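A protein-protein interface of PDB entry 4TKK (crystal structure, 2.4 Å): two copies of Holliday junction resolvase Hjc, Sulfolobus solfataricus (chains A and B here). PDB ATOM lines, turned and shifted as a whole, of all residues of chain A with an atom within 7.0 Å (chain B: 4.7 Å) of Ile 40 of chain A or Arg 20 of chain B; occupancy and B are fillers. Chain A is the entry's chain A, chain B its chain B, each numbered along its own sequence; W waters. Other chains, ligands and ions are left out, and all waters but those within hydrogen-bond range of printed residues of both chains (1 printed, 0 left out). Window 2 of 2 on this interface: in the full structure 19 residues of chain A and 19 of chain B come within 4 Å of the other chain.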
ATOM      1  N   ARG A  28      16.120   7.647 -23.332  1.00  0.00           N
ATOM      2  CA  ARG A  28      15.581   8.335 -24.489  1.00  0.00           C
ATOM      3  C   ARG A  28      15.413   7.284 -25.580  1.00  0.00           C
ATOM      4  O   ARG A  28      16.308   6.463 -25.804  1.00  0.00           O
ATOM      5  CB  ARG A  28      16.520   9.440 -24.950  1.00  0.00           C
ATOM      6  CG  ARG A  28      16.348  10.713 -24.136  1.00  0.00           C
ATOM      7  CD  ARG A  28      17.222  11.839 -24.636  1.00  0.00           C
ATOM      8  NE  ARG A  28      16.742  12.372 -25.911  1.00  0.00           N
ATOM      9  CZ  ARG A  28      17.512  12.562 -26.976  1.00  0.00           C
ATOM     10  NH1 ARG A  28      18.809  12.288 -26.923  1.00  0.00           N
ATOM     11  NH2 ARG A  28      16.993  13.033 -28.102  1.00  0.00           N
ATOM     12  N   ALA A  29      14.244   7.248 -26.211  1.00  0.00           N
ATOM     13  CA  ALA A  29      13.997   6.278 -27.268  1.00  0.00           C
ATOM     14  C   ALA A  29      14.997   6.490 -28.397  1.00  0.00           C
ATOM     15  O   ALA A  29      15.216   7.636 -28.798  1.00  0.00           O
ATOM     16  CB  ALA A  29      12.593   6.434 -27.800  1.00  0.00           C
ATOM     17  N   PRO A  30      15.633   5.425 -28.914  1.00  0.00           N
ATOM     18  CA  PRO A  30      16.553   5.629 -30.051  1.00  0.00           C
ATOM     19  C   PRO A  30      15.827   6.023 -31.346  1.00  0.00           C
ATOM     20  O   PRO A  30      14.589   5.963 -31.416  1.00  0.00           O
ATOM     21  CB  PRO A  30      17.310   4.304 -30.170  1.00  0.00           C
ATOM     22  CG  PRO A  30      16.562   3.323 -29.353  1.00  0.00           C
ATOM     23  CD  PRO A  30      15.494   3.994 -28.562  1.00  0.00           C
ATOM     24  N   LYS A  37      10.214   0.074 -36.579  1.00  0.00           N
ATOM     25  CA  LYS A  37       8.959   0.517 -37.181  1.00  0.00           C
ATOM     26  C   LYS A  37       7.913   1.040 -36.170  1.00  0.00           C
ATOM     27  O   LYS A  37       7.334   2.108 -36.410  1.00  0.00           O
ATOM     28  CB  LYS A  37       8.353  -0.561 -38.112  1.00  0.00           C
ATOM     29  CG  LYS A  37       8.131  -1.945 -37.472  1.00  0.00           C
ATOM     30  CD  LYS A  37       7.111  -2.787 -38.245  1.00  0.00           C
ATOM     31  CE  LYS A  37       5.774  -2.892 -37.545  1.00  0.00           C
ATOM     32  NZ  LYS A  37       5.798  -3.900 -36.451  1.00  0.00           N
ATOM     33  N   ASP A  38       7.652   0.279 -35.070  1.00  0.00           N
ATOM     34  CA  ASP A  38       6.663   0.621 -34.039  1.00  0.00           C
ATOM     35  C   ASP A  38       7.121   1.767 -33.124  1.00  0.00           C
ATOM     36  O   ASP A  38       8.248   1.717 -32.630  1.00  0.00           O
ATOM     37  CB  ASP A  38       6.246  -0.618 -33.233  1.00  0.00           C
ATOM     38  CG  ASP A  38       5.000  -1.330 -33.749  1.00  0.00           C
ATOM     39  OD1 ASP A  38       4.505  -0.958 -34.844  1.00  0.00           O
ATOM     40  OD2 ASP A  38       4.515  -2.256 -33.054  1.00  0.00           O
ATOM     41  N   PRO A  39       6.295   2.823 -32.911  1.00  0.00           N
ATOM     42  CA  PRO A  39       6.761   3.950 -32.089  1.00  0.00           C
ATOM     43  C   PRO A  39       6.974   3.651 -30.614  1.00  0.00           C
ATOM     44  O   PRO A  39       6.200   2.927 -29.995  1.00  0.00           O
ATOM     45  CB  PRO A  39       5.711   5.040 -32.313  1.00  0.00           C
ATOM     46  CG  PRO A  39       4.569   4.396 -32.905  1.00  0.00           C
ATOM     47  CD  PRO A  39       4.934   3.057 -33.435  1.00  0.00           C
ATOM     48  N   ILE A  40       8.069   4.187 -30.078  1.00  0.00           N
ATOM     49  CA  ILE A  40       8.479   4.122 -28.678  1.00  0.00           C
ATOM     50  C   ILE A  40       8.372   5.561 -28.194  1.00  0.00           C
ATOM     51  O   ILE A  40       8.910   6.425 -28.869  1.00  0.00           O
ATOM     52  CB  ILE A  40       9.933   3.565 -28.528  1.00  0.00           C
ATOM     53  CG1 ILE A  40      10.037   2.122 -29.093  1.00  0.00           C
ATOM     54  CG2 ILE A  40      10.421   3.641 -27.071  1.00  0.00           C
ATOM     55  CD1 ILE A  40      11.456   1.559 -29.163  1.00  0.00           C
ATOM     56  N   PRO A  41       7.716   5.857 -27.042  1.00  0.00           N
ATOM     57  CA  PRO A  41       7.692   7.253 -26.549  1.00  0.00           C
ATOM     58  C   PRO A  41       9.106   7.802 -26.418  1.00  0.00           C
ATOM     59  O   PRO A  41      10.030   7.046 -26.108  1.00  0.00           O
ATOM     60  CB  PRO A  41       7.004   7.142 -25.186  1.00  0.00           C
ATOM     61  CG  PRO A  41       6.212   5.891 -25.264  1.00  0.00           C
ATOM     62  CD  PRO A  41       7.045   4.954 -26.084  1.00  0.00           C
ATOM     63  N   ASP A  42       9.285   9.096 -26.730  1.00  0.00           N
ATOM     64  CA  ASP A  42      10.588   9.770 -26.709  1.00  0.00           C
ATOM     65  C   ASP A  42      11.364   9.559 -25.437  1.00  0.00           C
ATOM     66  O   ASP A  42      12.547   9.253 -25.489  1.00  0.00           O
ATOM     67  CB  ASP A  42      10.429  11.270 -26.985  1.00  0.00           C
ATOM     68  CG  ASP A  42       9.821  11.534 -28.331  1.00  0.00           C
ATOM     69  OD1 ASP A  42      10.267  10.913 -29.301  1.00  0.00           O
ATOM     70  OD2 ASP A  42       8.922  12.394 -28.417  1.00  0.00           O
ATOM     71  N   ILE A  43      10.692   9.706 -24.302  1.00  0.00           N
ATOM     72  CA  ILE A  43      11.309   9.574 -22.988  1.00  0.00           C
ATOM     73  C   ILE A  43      10.599   8.507 -22.172  1.00  0.00           C
ATOM     74  O   ILE A  43       9.376   8.508 -22.060  1.00  0.00           O
ATOM     75  CB  ILE A  43      11.355  10.960 -22.265  1.00  0.00           C
ATOM     76  CG1 ILE A  43      12.178  11.995 -23.090  1.00  0.00           C
ATOM     77  CG2 ILE A  43      11.862  10.843 -20.819  1.00  0.00           C
ATOM     78  CD1 ILE A  43      12.000  13.448 -22.676  1.00  0.00           C
ATOM     79  N   ILE A  44      11.390   7.624 -21.574  1.00  0.00           N
ATOM     80  CA  ILE A  44      10.927   6.593 -20.666  1.00  0.00           C
ATOM     81  C   ILE A  44      11.672   6.847 -19.359  1.00  0.00           C
ATOM     82  O   ILE A  44      12.897   6.815 -19.328  1.00  0.00           O
ATOM     83  CB  ILE A  44      11.154   5.174 -21.226  1.00  0.00           C
ATOM     84  CG1 ILE A  44      10.368   4.996 -22.536  1.00  0.00           C
ATOM     85  CG2 ILE A  44      10.777   4.107 -20.194  1.00  0.00           C
ATOM     86  CD1 ILE A  44      10.973   4.106 -23.457  1.00  0.00           C
ATOM     87  N   LEU A  53       5.955   7.774 -19.360  1.00  0.00           N
ATOM     88  CA  LEU A  53       6.287   7.820 -20.783  1.00  0.00           C
ATOM     89  C   LEU A  53       5.917   9.171 -21.250  1.00  0.00           C
ATOM     90  O   LEU A  53       4.821   9.639 -20.980  1.00  0.00           O
ATOM     91  CB  LEU A  53       5.529   6.701 -21.573  1.00  0.00           C
ATOM     92  CG  LEU A  53       5.647   5.320 -20.976  1.00  0.00           C
ATOM     93  CD1 LEU A  53       4.636   4.408 -21.544  1.00  0.00           C
ATOM     94  CD2 LEU A  53       7.079   4.765 -21.128  1.00  0.00           C
ATOM     95  N   ILE A  54       6.863   9.831 -21.878  1.00  0.00           N
ATOM     96  CA  ILE A  54       6.653  11.177 -22.359  1.00  0.00           C
ATOM     97  C   ILE A  54       6.923  11.276 -23.838  1.00  0.00           C
ATOM     98  O   ILE A  54       8.033  10.994 -24.314  1.00  0.00           O
ATOM     99  CB  ILE A  54       7.445  12.244 -21.556  1.00  0.00           C
ATOM    100  CG1 ILE A  54       7.045  12.242 -20.079  1.00  0.00           C
ATOM    101  CG2 ILE A  54       7.200  13.634 -22.165  1.00  0.00           C
ATOM    102  CD1 ILE A  54       8.146  12.889 -19.137  1.00  0.00           C
ATOM    103  N   GLU A  55       5.911  11.748 -24.551  1.00  0.00           N
ATOM    104  CA  GLU A  55       6.001  11.987 -25.975  1.00  0.00           C
ATOM    105  C   GLU A  55       6.266  13.473 -26.158  1.00  0.00           C
ATOM    106  O   GLU A  55       5.519  14.300 -25.653  1.00  0.00           O
ATOM    107  CB  GLU A  55       4.694  11.550 -26.679  1.00  0.00           C
ATOM    108  CG  GLU A  55       4.758  11.684 -28.189  1.00  0.00           C
ATOM    109  CD  GLU A  55       5.705  10.731 -28.887  1.00  0.00           C
ATOM    110  OE1 GLU A  55       6.494  10.041 -28.201  1.00  0.00           O
ATOM    111  OE2 GLU A  55       5.682  10.711 -30.137  1.00  0.00           O
ATOM    112  N   LYS A  57       7.193  14.768 -29.432  1.00  0.00           N
ATOM    113  CA  LYS A  57       6.767  15.047 -30.800  1.00  0.00           C
ATOM    114  C   LYS A  57       5.261  15.264 -30.825  1.00  0.00           C
ATOM    115  O   LYS A  57       4.511  14.582 -30.130  1.00  0.00           O
ATOM    116  CB  LYS A  57       7.066  13.856 -31.726  1.00  0.00           C
ATOM    117  CG  LYS A  57       8.510  13.408 -31.838  1.00  0.00           C
ATOM    118  CD  LYS A  57       8.663  12.256 -32.846  1.00  0.00           C
ATOM    119  CE  LYS A  57       8.033  10.931 -32.433  1.00  0.00           C
ATOM    120  NZ  LYS A  57       8.838  10.199 -31.421  1.00  0.00           N
ATOM    121  N   GLN A  72       0.970   7.222 -34.890  1.00  0.00           N
ATOM    122  CA  GLN A  72       1.947   7.563 -33.870  1.00  0.00           C
ATOM    123  C   GLN A  72       1.293   7.413 -32.495  1.00  0.00           C
ATOM    124  O   GLN A  72       1.844   6.747 -31.621  1.00  0.00           O
ATOM    125  CB  GLN A  72       2.494   8.994 -34.050  1.00  0.00           C
ATOM    126  CG  GLN A  72       3.493   9.399 -32.917  1.00  0.00           C
ATOM    127  CD  GLN A  72       4.762   8.567 -32.872  1.00  0.00           C
ATOM    128  OE1 GLN A  72       5.138   7.925 -33.850  1.00  0.00           O
ATOM    129  NE2 GLN A  72       5.479   8.562 -31.747  1.00  0.00           N
ATOM    130  N   GLY A  75       0.548   3.718 -31.489  1.00  0.00           N
ATOM    131  CA  GLY A  75       1.798   3.033 -31.180  1.00  0.00           C
ATOM    132  C   GLY A  75       2.307   3.332 -29.781  1.00  0.00           C
ATOM    133  O   GLY A  75       2.646   2.413 -29.026  1.00  0.00           O
ATOM    134  N   ILE A  76       2.302   4.614 -29.406  1.00  0.00           N
ATOM    135  CA  ILE A  76       2.742   5.041 -28.073  1.00  0.00           C
ATOM    136  C   ILE A  76       1.716   4.684 -27.025  1.00  0.00           C
ATOM    137  O   ILE A  76       2.101   4.366 -25.908  1.00  0.00           O
ATOM    138  CB  ILE A  76       3.243   6.507 -28.024  1.00  0.00           C
ATOM    139  CG1 ILE A  76       2.103   7.523 -28.333  1.00  0.00           C
ATOM    140  CG2 ILE A  76       4.457   6.670 -28.967  1.00  0.00           C
ATOM    141  CD1 ILE A  76       2.411   8.925 -28.227  1.00  0.00           C
ATOM    142  N   PHE A  79       2.423   1.061 -26.495  1.00  0.00           N
ATOM    143  CA  PHE A  79       3.624   0.951 -25.667  1.00  0.00           C
ATOM    144  C   PHE A  79       3.257   1.197 -24.194  1.00  0.00           C
ATOM    145  O   PHE A  79       3.668   0.437 -23.311  1.00  0.00           O
ATOM    146  CB  PHE A  79       4.692   1.942 -26.133  1.00  0.00           C
ATOM    147  CG  PHE A  79       6.046   1.676 -25.524  1.00  0.00           C
ATOM    148  CD1 PHE A  79       6.334   2.081 -24.224  1.00  0.00           C
ATOM    149  CD2 PHE A  79       7.049   1.065 -26.264  1.00  0.00           C
ATOM    150  CE1 PHE A  79       7.578   1.820 -23.651  1.00  0.00           C
ATOM    151  CE2 PHE A  79       8.318   0.852 -25.711  1.00  0.00           C
ATOM    152  CZ  PHE A  79       8.574   1.230 -24.404  1.00  0.00           C
ATOM    153  N   LYS A  82       0.860  -1.691 -22.815  1.00  0.00           N
ATOM    154  CA  LYS A  82       1.633  -2.903 -22.576  1.00  0.00           C
ATOM    155  C   LYS A  82       2.564  -2.772 -21.376  1.00  0.00           C
ATOM    156  O   LYS A  82       2.645  -3.682 -20.545  1.00  0.00           O
ATOM    157  CB  LYS A  82       2.456  -3.262 -23.808  1.00  0.00           C
ATOM    158  CG  LYS A  82       1.634  -3.754 -24.962  1.00  0.00           C
ATOM    159  CD  LYS A  82       2.572  -3.970 -26.130  1.00  0.00           C
ATOM    160  CE  LYS A  82       1.891  -4.711 -27.229  1.00  0.00           C
ATOM    161  NZ  LYS A  82       2.746  -4.785 -28.437  1.00  0.00           N
ATOM    162  N   VAL B  16      14.648  -8.778 -28.177  1.00  0.00           N
ATOM    163  CA  VAL B  16      13.692  -7.674 -28.289  1.00  0.00           C
ATOM    164  C   VAL B  16      12.431  -8.137 -29.005  1.00  0.00           C
ATOM    165  O   VAL B  16      11.327  -7.956 -28.488  1.00  0.00           O
ATOM    166  CB  VAL B  16      14.360  -6.455 -28.984  1.00  0.00           C
ATOM    167  CG1 VAL B  16      13.340  -5.398 -29.359  1.00  0.00           C
ATOM    168  CG2 VAL B  16      15.430  -5.853 -28.092  1.00  0.00           C
ATOM    169  N   SER B  17      12.616  -8.796 -30.162  1.00  0.00           N
ATOM    170  CA  SER B  17      11.562  -9.338 -31.018  1.00  0.00           C
ATOM    171  C   SER B  17      10.744 -10.342 -30.245  1.00  0.00           C
ATOM    172  O   SER B  17       9.519 -10.242 -30.200  1.00  0.00           O
ATOM    173  CB  SER B  17      12.178  -9.969 -32.261  1.00  0.00           C
ATOM    174  OG  SER B  17      11.183 -10.294 -33.216  1.00  0.00           O
ATOM    175  N   ARG B  18      11.420 -11.214 -29.525  1.00  0.00           N
ATOM    176  CA  ARG B  18      10.765 -12.227 -28.711  1.00  0.00           C
ATOM    177  C   ARG B  18      10.019 -11.655 -27.527  1.00  0.00           C
ATOM    178  O   ARG B  18       8.907 -12.095 -27.234  1.00  0.00           O
ATOM    179  CB  ARG B  18      11.776 -13.288 -28.289  1.00  0.00           C
ATOM    180  CG  ARG B  18      12.231 -14.119 -29.483  1.00  0.00           C
ATOM    181  CD  ARG B  18      13.579 -14.741 -29.240  1.00  0.00           C
ATOM    182  NE  ARG B  18      13.526 -15.726 -28.168  1.00  0.00           N
ATOM    183  CZ  ARG B  18      14.588 -16.349 -27.691  1.00  0.00           C
ATOM    184  NH1 ARG B  18      15.798 -16.068 -28.161  1.00  0.00           N
ATOM    185  NH2 ARG B  18      14.455 -17.241 -26.719  1.00  0.00           N
ATOM    186  N   LEU B  19      10.597 -10.651 -26.860  1.00  0.00           N
ATOM    187  CA  LEU B  19       9.915 -10.014 -25.732  1.00  0.00           C
ATOM    188  C   LEU B  19       8.736  -9.199 -26.243  1.00  0.00           C
ATOM    189  O   LEU B  19       7.686  -9.230 -25.631  1.00  0.00           O
ATOM    190  CB  LEU B  19      10.878  -9.158 -24.887  1.00  0.00           C
ATOM    191  CG  LEU B  19      11.838  -9.923 -23.991  1.00  0.00           C
ATOM    192  CD1 LEU B  19      12.893  -9.026 -23.467  1.00  0.00           C
ATOM    193  CD2 LEU B  19      11.109 -10.632 -22.860  1.00  0.00           C
ATOM    194  N   ARG B  20       8.875  -8.546 -27.395  1.00  0.00           N
ATOM    195  CA  ARG B  20       7.752  -7.818 -28.006  1.00  0.00           C
ATOM    196  C   ARG B  20       6.589  -8.773 -28.345  1.00  0.00           C
ATOM    197  O   ARG B  20       5.439  -8.452 -28.033  1.00  0.00           O
ATOM    198  CB  ARG B  20       8.194  -7.028 -29.237  1.00  0.00           C
ATOM    199  CG  ARG B  20       8.797  -5.695 -28.876  1.00  0.00           C
ATOM    200  CD  ARG B  20       9.320  -4.901 -30.067  1.00  0.00           C
ATOM    201  NE  ARG B  20       9.876  -3.636 -29.593  1.00  0.00           N
ATOM    202  CZ  ARG B  20      10.917  -3.014 -30.128  1.00  0.00           C
ATOM    203  NH1 ARG B  20      11.525  -3.517 -31.190  1.00  0.00           N
ATOM    204  NH2 ARG B  20      11.350  -1.875 -29.616  1.00  0.00           N
ATOM    205  N   ASP B  21       6.894  -9.979 -28.888  1.00  0.00           N
ATOM    206  CA  ASP B  21       5.884 -11.018 -29.202  1.00  0.00           C
ATOM    207  C   ASP B  21       5.187 -11.495 -27.946  1.00  0.00           C
ATOM    208  O   ASP B  21       4.058 -11.982 -28.006  1.00  0.00           O
ATOM    209  CB  ASP B  21       6.531 -12.231 -29.883  1.00  0.00           C
ATOM    210  CG  ASP B  21       7.072 -11.998 -31.280  1.00  0.00           C
ATOM    211  OD1 ASP B  21       6.662 -11.009 -31.922  1.00  0.00           O
ATOM    212  OD2 ASP B  21       7.912 -12.803 -31.730  1.00  0.00           O
ATOM    213  N   LYS B  22       5.872 -11.376 -26.809  1.00  0.00           N
ATOM    214  CA  LYS B  22       5.355 -11.781 -25.513  1.00  0.00           C
ATOM    215  C   LYS B  22       4.563 -10.676 -24.808  1.00  0.00           C
ATOM    216  O   LYS B  22       4.201 -10.825 -23.650  1.00  0.00           O
ATOM    217  CB  LYS B  22       6.509 -12.298 -24.676  1.00  0.00           C
ATOM    218  CG  LYS B  22       6.348 -13.748 -24.281  1.00  0.00           C
ATOM    219  CD  LYS B  22       6.655 -14.755 -25.364  1.00  0.00           C
ATOM    220  CE  LYS B  22       5.828 -15.993 -25.136  1.00  0.00           C
ATOM    221  NZ  LYS B  22       6.286 -16.761 -23.951  1.00  0.00           N
ATOM    222  N   GLY B  23       4.284  -9.592 -25.530  1.00  0.00           N
ATOM    223  CA  GLY B  23       3.514  -8.463 -25.036  1.00  0.00           C
ATOM    224  C   GLY B  23       4.297  -7.421 -24.256  1.00  0.00           C
ATOM    225  O   GLY B  23       3.689  -6.625 -23.540  1.00  0.00           O
ATOM    226  N   PHE B  24       5.642  -7.415 -24.362  1.00  0.00           N
ATOM    227  CA  PHE B  24       6.441  -6.423 -23.637  1.00  0.00           C
ATOM    228  C   PHE B  24       6.615  -5.173 -24.460  1.00  0.00           C
ATOM    229  O   PHE B  24       6.771  -5.264 -25.678  1.00  0.00           O
ATOM    230  CB  PHE B  24       7.844  -6.962 -23.285  1.00  0.00           C
ATOM    231  CG  PHE B  24       7.901  -7.967 -22.168  1.00  0.00           C
ATOM    232  CD1 PHE B  24       7.511  -9.289 -22.380  1.00  0.00           C
ATOM    233  CD2 PHE B  24       8.376  -7.608 -20.910  1.00  0.00           C
ATOM    234  CE1 PHE B  24       7.577 -10.230 -21.346  1.00  0.00           C
ATOM    235  CE2 PHE B  24       8.420  -8.540 -19.869  1.00  0.00           C
ATOM    236  CZ  PHE B  24       8.031  -9.849 -20.097  1.00  0.00           C
ATOM    237  N   VAL B  26       9.272  -2.780 -25.334  1.00  0.00           N
ATOM    238  CA  VAL B  26      10.711  -2.945 -25.290  1.00  0.00           C
ATOM    239  C   VAL B  26      11.423  -1.774 -25.886  1.00  0.00           C
ATOM    240  O   VAL B  26      10.983  -1.222 -26.897  1.00  0.00           O
ATOM    241  CB  VAL B  26      11.172  -4.275 -25.942  1.00  0.00           C
ATOM    242  CG1 VAL B  26      12.664  -4.532 -25.706  1.00  0.00           C
ATOM    243  CG2 VAL B  26      10.342  -5.462 -25.438  1.00  0.00           C
ATOM    244  N   VAL B  27      12.531  -1.391 -25.248  1.00  0.00           N
ATOM    245  CA  VAL B  27      13.399  -0.339 -25.731  1.00  0.00           C
ATOM    246  C   VAL B  27      14.874  -0.776 -25.581  1.00  0.00           C
ATOM    247  O   VAL B  27      15.269  -1.359 -24.566  1.00  0.00           O
ATOM    248  CB  VAL B  27      13.057   1.074 -25.169  1.00  0.00           C
ATOM    249  CG1 VAL B  27      13.222   1.156 -23.653  1.00  0.00           C
ATOM    250  CG2 VAL B  27      13.872   2.160 -25.858  1.00  0.00           C
HETATM  251  O   HOH W   1       9.910  -0.218 -32.101  1.00  0.00           O
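Arg 20 of chain B touches just one residue of chain A: Ile 40 (3.5 Å). Of the printed residues of chain A, Gly 23 of chain B touches Lys 82 (3.6 Å). Of the printed residues of chain A, Val 27 of chain B touches Pro 30 (3.6 Å), Ile 40 (3.9 Å) and Ile 44 (3.7 Å). Of the printed residues of chain A, Val 26 of chain B touches Ile 40 (3.6 Å) and Phe 79 (3.6 Å). Printed residues of chain B within 4 Å of Ile 44 of chain A: Val 27. Printed residues of chain B within 4 Å of Lys 82 of chain A: Gly 23 (3.6 Å). Lys 37 of chain A touches none of the printed residues of chain B. Gln 72 of chain A touches none of the printed residues of chain B. The nearest printed residue of chain B that does not touch Ile 40 of chain A is Val 16 of chain B (7.2 Å). The nearest residue of chain A that does not touch Arg 20 of chain B is Lys 82 of chain A (4.6 Å).
Water W1 lies within hydrogen-bond range of O of Asp 38 of chain A (2.6 Å) and NH2 of Arg 20 of chain B (3.3 Å).
The guanidinium group (NH2) of Arg 20 of chain B lies within hydrogen-bond range of the backbone carbonyl oxygen (O) of Val 26 of chain B.
Of the 20 printed residues of chain A, 5 touch a printed residue of chain B. Hydrophobic or aromatic side chains of chain A that line the printed part of chain B: Pro 30, Ile 40, Ile 44 and Phe 79. Along chain A the printed residues that touch a printed residue of chain B span positions 30 to 82. Hydrophobic or aromatic side chains of chain B within 4 Å of the printed part of chain A: Val 27. Among the printed residues, no Asp or Glu carboxylate lies within 4 Å of a Lys or Arg side-chain nitrogen of the other chain.
No position is printed for both chains. Of the 7 pairs that touch across the chains among the printed residues, none has its exchanged pair printed and touching as well.
CG2 of Val 27 of chain B touches CD of Pro 30 of chain A, at 3.6 Å. Ile 40 of chain A touches Arg 20 of chain B (CD1 to NH2, 3.5 Å). Val 26 of chain B touches Ile 40 of chain A. CG2 of Ile 40 of chain A touches CG2 of Val 27 of chain B, at 3.9 Å. Val 27 of chain B touches Ile 44 of chain A. Val 26 of chain B touches Phe 79 of chain A (O to CE2, 3.6 Å). Lys 82 of chain A touches Gly 23 of chain B.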
